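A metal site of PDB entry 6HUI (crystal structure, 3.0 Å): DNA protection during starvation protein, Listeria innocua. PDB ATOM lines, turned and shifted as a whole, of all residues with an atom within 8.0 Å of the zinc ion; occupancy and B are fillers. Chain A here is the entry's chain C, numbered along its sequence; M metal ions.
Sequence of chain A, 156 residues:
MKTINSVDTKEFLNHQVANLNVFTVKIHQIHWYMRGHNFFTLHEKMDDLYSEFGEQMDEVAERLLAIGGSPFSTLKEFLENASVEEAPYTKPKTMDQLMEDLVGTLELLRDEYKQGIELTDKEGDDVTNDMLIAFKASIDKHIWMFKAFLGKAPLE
Within 4 Å of the zinc ion: His 15, Ser 83 and Glu 112. The nearest printed residue that does not touch the zinc ion is Asn 19 (4.6 Å).
The zinc ion is bound by NE2 of His 15, 2.2 Å away. The side-chain carboxylate (OE2) of Glu 112 binds the zinc ion (2.3 Å). The zinc ion is bound by OG of Ser 83 (2.6 Å). The zinc ion has three donor atoms within binding distance.
The side-chain amide nitrogen of Gln 16 sits at hydrogen-bond distance from the side-chain carboxylate of Glu 112 (2.6 Å). The side-chain carboxylate (OE1) of Glu 112 lies within hydrogen-bond range of the side-chain amide nitrogen (ND2) of Asn 19 (3.4 Å). The backbone carbonyl oxygen (O) of Asn 81 lies within hydrogen-bond range of a ring nitrogen (ND1) of His 15 (2.9 Å). ND2 of Asn 19 lies within hydrogen-bond range of O of His 15 (2.9 Å). The backbone NH of Ser 83 sits at hydrogen-bond distance from the side-chain amide oxygen of Asn 19.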
ATOM      1  N   PHE A  12     -13.046  -2.162  36.268  1.00  0.00           N
ATOM      2  CA  PHE A  12     -13.923  -1.361  35.415  1.00  0.00           C
ATOM      3  C   PHE A  12     -13.327   0.027  35.168  1.00  0.00           C
ATOM      4  O   PHE A  12     -13.352   0.513  34.035  1.00  0.00           O
ATOM      5  CB  PHE A  12     -15.315  -1.252  36.038  1.00  0.00           C
ATOM      6  CG  PHE A  12     -16.247  -0.360  35.286  1.00  0.00           C
ATOM      7  CD1 PHE A  12     -16.917  -0.822  34.166  1.00  0.00           C
ATOM      8  CD2 PHE A  12     -16.456   0.953  35.683  1.00  0.00           C
ATOM      9  CE1 PHE A  12     -17.780  -0.002  33.463  1.00  0.00           C
ATOM     10  CE2 PHE A  12     -17.318   1.779  34.987  1.00  0.00           C
ATOM     11  CZ  PHE A  12     -17.976   1.303  33.875  1.00  0.00           C
ATOM     12  N   HIS A  15     -10.433  -0.296  32.791  1.00  0.00           N
ATOM     13  CA  HIS A  15     -11.007  -0.580  31.480  1.00  0.00           C
ATOM     14  C   HIS A  15     -11.498   0.702  30.816  1.00  0.00           C
ATOM     15  O   HIS A  15     -11.233   0.956  29.635  1.00  0.00           O
ATOM     16  CB  HIS A  15     -12.149  -1.590  31.635  1.00  0.00           C
ATOM     17  CG  HIS A  15     -12.644  -2.153  30.334  1.00  0.00           C
ATOM     18  ND1 HIS A  15     -11.872  -2.182  29.196  1.00  0.00           N
ATOM     19  CD2 HIS A  15     -13.826  -2.719  30.002  1.00  0.00           C
ATOM     20  CE1 HIS A  15     -12.571  -2.734  28.219  1.00  0.00           C
ATOM     21  NE2 HIS A  15     -13.758  -3.070  28.685  1.00  0.00           N
ATOM     22  N   GLN A  16     -12.217   1.537  31.576  1.00  0.00           N
ATOM     23  CA  GLN A  16     -12.705   2.803  31.041  1.00  0.00           C
ATOM     24  C   GLN A  16     -11.582   3.815  30.838  1.00  0.00           C
ATOM     25  O   GLN A  16     -11.744   4.736  30.032  1.00  0.00           O
ATOM     26  CB  GLN A  16     -13.767   3.390  31.963  1.00  0.00           C
ATOM     27  CG  GLN A  16     -15.003   2.504  32.128  1.00  0.00           C
ATOM     28  CD  GLN A  16     -15.697   2.212  30.806  1.00  0.00           C
ATOM     29  OE1 GLN A  16     -15.624   2.991  29.860  1.00  0.00           O
ATOM     30  NE2 GLN A  16     -16.375   1.071  30.744  1.00  0.00           N
ATOM     31  N   ASN A  19     -10.471   2.690  27.412  1.00  0.00           N
ATOM     32  CA  ASN A  19     -11.519   3.092  26.476  1.00  0.00           C
ATOM     33  C   ASN A  19     -11.502   4.598  26.229  1.00  0.00           C
ATOM     34  O   ASN A  19     -11.690   5.045  25.097  1.00  0.00           O
ATOM     35  CB  ASN A  19     -12.887   2.672  27.020  1.00  0.00           C
ATOM     36  CG  ASN A  19     -13.046   1.174  27.081  1.00  0.00           C
ATOM     37  OD1 ASN A  19     -12.570   0.443  26.209  1.00  0.00           O
ATOM     38  ND2 ASN A  19     -13.725   0.693  28.119  1.00  0.00           N
ATOM     39  N   ASN A  81      -6.236  -3.688  26.682  1.00  0.00           N
ATOM     40  CA  ASN A  81      -7.411  -3.810  27.536  1.00  0.00           C
ATOM     41  C   ASN A  81      -8.626  -3.029  27.056  1.00  0.00           C
ATOM     42  O   ASN A  81      -9.724  -3.239  27.592  1.00  0.00           O
ATOM     43  CB  ASN A  81      -7.077  -3.366  28.975  1.00  0.00           C
ATOM     44  CG  ASN A  81      -8.038  -3.948  30.005  1.00  0.00           C
ATOM     45  OD1 ASN A  81      -8.610  -3.223  30.806  1.00  0.00           O
ATOM     46  ND2 ASN A  81      -8.207  -5.266  29.969  1.00  0.00           N
ATOM     47  N   ALA A  82      -8.484  -2.138  26.080  1.00  0.00           N
ATOM     48  CA  ALA A  82      -9.623  -1.335  25.652  1.00  0.00           C
ATOM     49  C   ALA A  82     -10.612  -2.169  24.849  1.00  0.00           C
ATOM     50  O   ALA A  82     -10.226  -3.039  24.071  1.00  0.00           O
ATOM     51  CB  ALA A  82      -9.156  -0.135  24.823  1.00  0.00           C
ATOM     52  N   SER A  83     -11.899  -1.894  25.053  1.00  0.00           N
ATOM     53  CA  SER A  83     -12.966  -2.512  24.274  1.00  0.00           C
ATOM     54  C   SER A  83     -13.500  -1.607  23.175  1.00  0.00           C
ATOM     55  O   SER A  83     -14.443  -1.993  22.478  1.00  0.00           O
ATOM     56  CB  SER A  83     -14.114  -2.945  25.191  1.00  0.00           C
ATOM     57  OG  SER A  83     -14.640  -1.833  25.901  1.00  0.00           O
ATOM     58  N   VAL A  84     -12.935  -0.414  23.009  1.00  0.00           N
ATOM     59  CA  VAL A  84     -13.325   0.501  21.938  1.00  0.00           C
ATOM     60  C   VAL A  84     -12.453   0.223  20.729  1.00  0.00           C
ATOM     61  O   VAL A  84     -11.227   0.133  20.841  1.00  0.00           O
ATOM     62  CB  VAL A  84     -13.200   1.960  22.397  1.00  0.00           C
ATOM     63  CG1 VAL A  84     -13.516   2.911  21.250  1.00  0.00           C
ATOM     64  CG2 VAL A  84     -14.113   2.233  23.582  1.00  0.00           C
ATOM     65  N   LEU A 108     -21.487   2.873  23.074  1.00  0.00           N
ATOM     66  CA  LEU A 108     -20.682   1.891  23.803  1.00  0.00           C
ATOM     67  C   LEU A 108     -20.376   2.381  25.215  1.00  0.00           C
ATOM     68  O   LEU A 108     -20.633   1.678  26.196  1.00  0.00           O
ATOM     69  CB  LEU A 108     -19.400   1.606  23.024  1.00  0.00           C
ATOM     70  CG  LEU A 108     -18.471   0.445  23.401  1.00  0.00           C
ATOM     71  CD1 LEU A 108     -17.643   0.048  22.194  1.00  0.00           C
ATOM     72  CD2 LEU A 108     -17.567   0.801  24.559  1.00  0.00           C
ATOM     73  N   LEU A 109     -19.849   3.602  25.324  1.00  0.00           N
ATOM     74  CA  LEU A 109     -19.547   4.152  26.640  1.00  0.00           C
ATOM     75  C   LEU A 109     -20.811   4.364  27.469  1.00  0.00           C
ATOM     76  O   LEU A 109     -20.766   4.315  28.700  1.00  0.00           O
ATOM     77  CB  LEU A 109     -18.769   5.458  26.506  1.00  0.00           C
ATOM     78  CG  LEU A 109     -17.364   5.330  25.907  1.00  0.00           C
ATOM     79  CD1 LEU A 109     -16.675   6.681  25.869  1.00  0.00           C
ATOM     80  CD2 LEU A 109     -16.538   4.322  26.689  1.00  0.00           C
ATOM     81  N   GLU A 112     -21.627   0.685  28.810  1.00  0.00           N
ATOM     82  CA  GLU A 112     -20.626   0.280  29.788  1.00  0.00           C
ATOM     83  C   GLU A 112     -20.693   1.139  31.052  1.00  0.00           C
ATOM     84  O   GLU A 112     -20.569   0.617  32.170  1.00  0.00           O
ATOM     85  CB  GLU A 112     -19.229   0.337  29.179  1.00  0.00           C
ATOM     86  CG  GLU A 112     -18.989  -0.704  28.097  1.00  0.00           C
ATOM     87  CD  GLU A 112     -17.534  -1.123  28.019  1.00  0.00           C
ATOM     88  OE1 GLU A 112     -16.740  -0.703  28.887  1.00  0.00           O
ATOM     89  OE2 GLU A 112     -17.180  -1.878  27.084  1.00  0.00           O
ATOM     90  N   GLN A 115     -23.530  -0.110  33.159  1.00  0.00           N
ATOM     91  CA  GLN A 115     -23.100  -1.289  33.903  1.00  0.00           C
ATOM     92  C   GLN A 115     -22.237  -0.909  35.095  1.00  0.00           C
ATOM     93  O   GLN A 115     -22.362  -1.506  36.176  1.00  0.00           O
ATOM     94  CB  GLN A 115     -22.350  -2.255  32.976  1.00  0.00           C
ATOM     95  CG  GLN A 115     -23.208  -2.872  31.889  1.00  0.00           C
ATOM     96  CD  GLN A 115     -22.426  -3.808  30.994  1.00  0.00           C
ATOM     97  OE1 GLN A 115     -21.204  -3.910  31.090  1.00  0.00           O
ATOM     98  NE2 GLN A 115     -23.135  -4.506  30.107  1.00  0.00           N
HETATM   99 ZN    ZN M   1     -15.650  -3.447  27.650  1.00  0.00          ZN
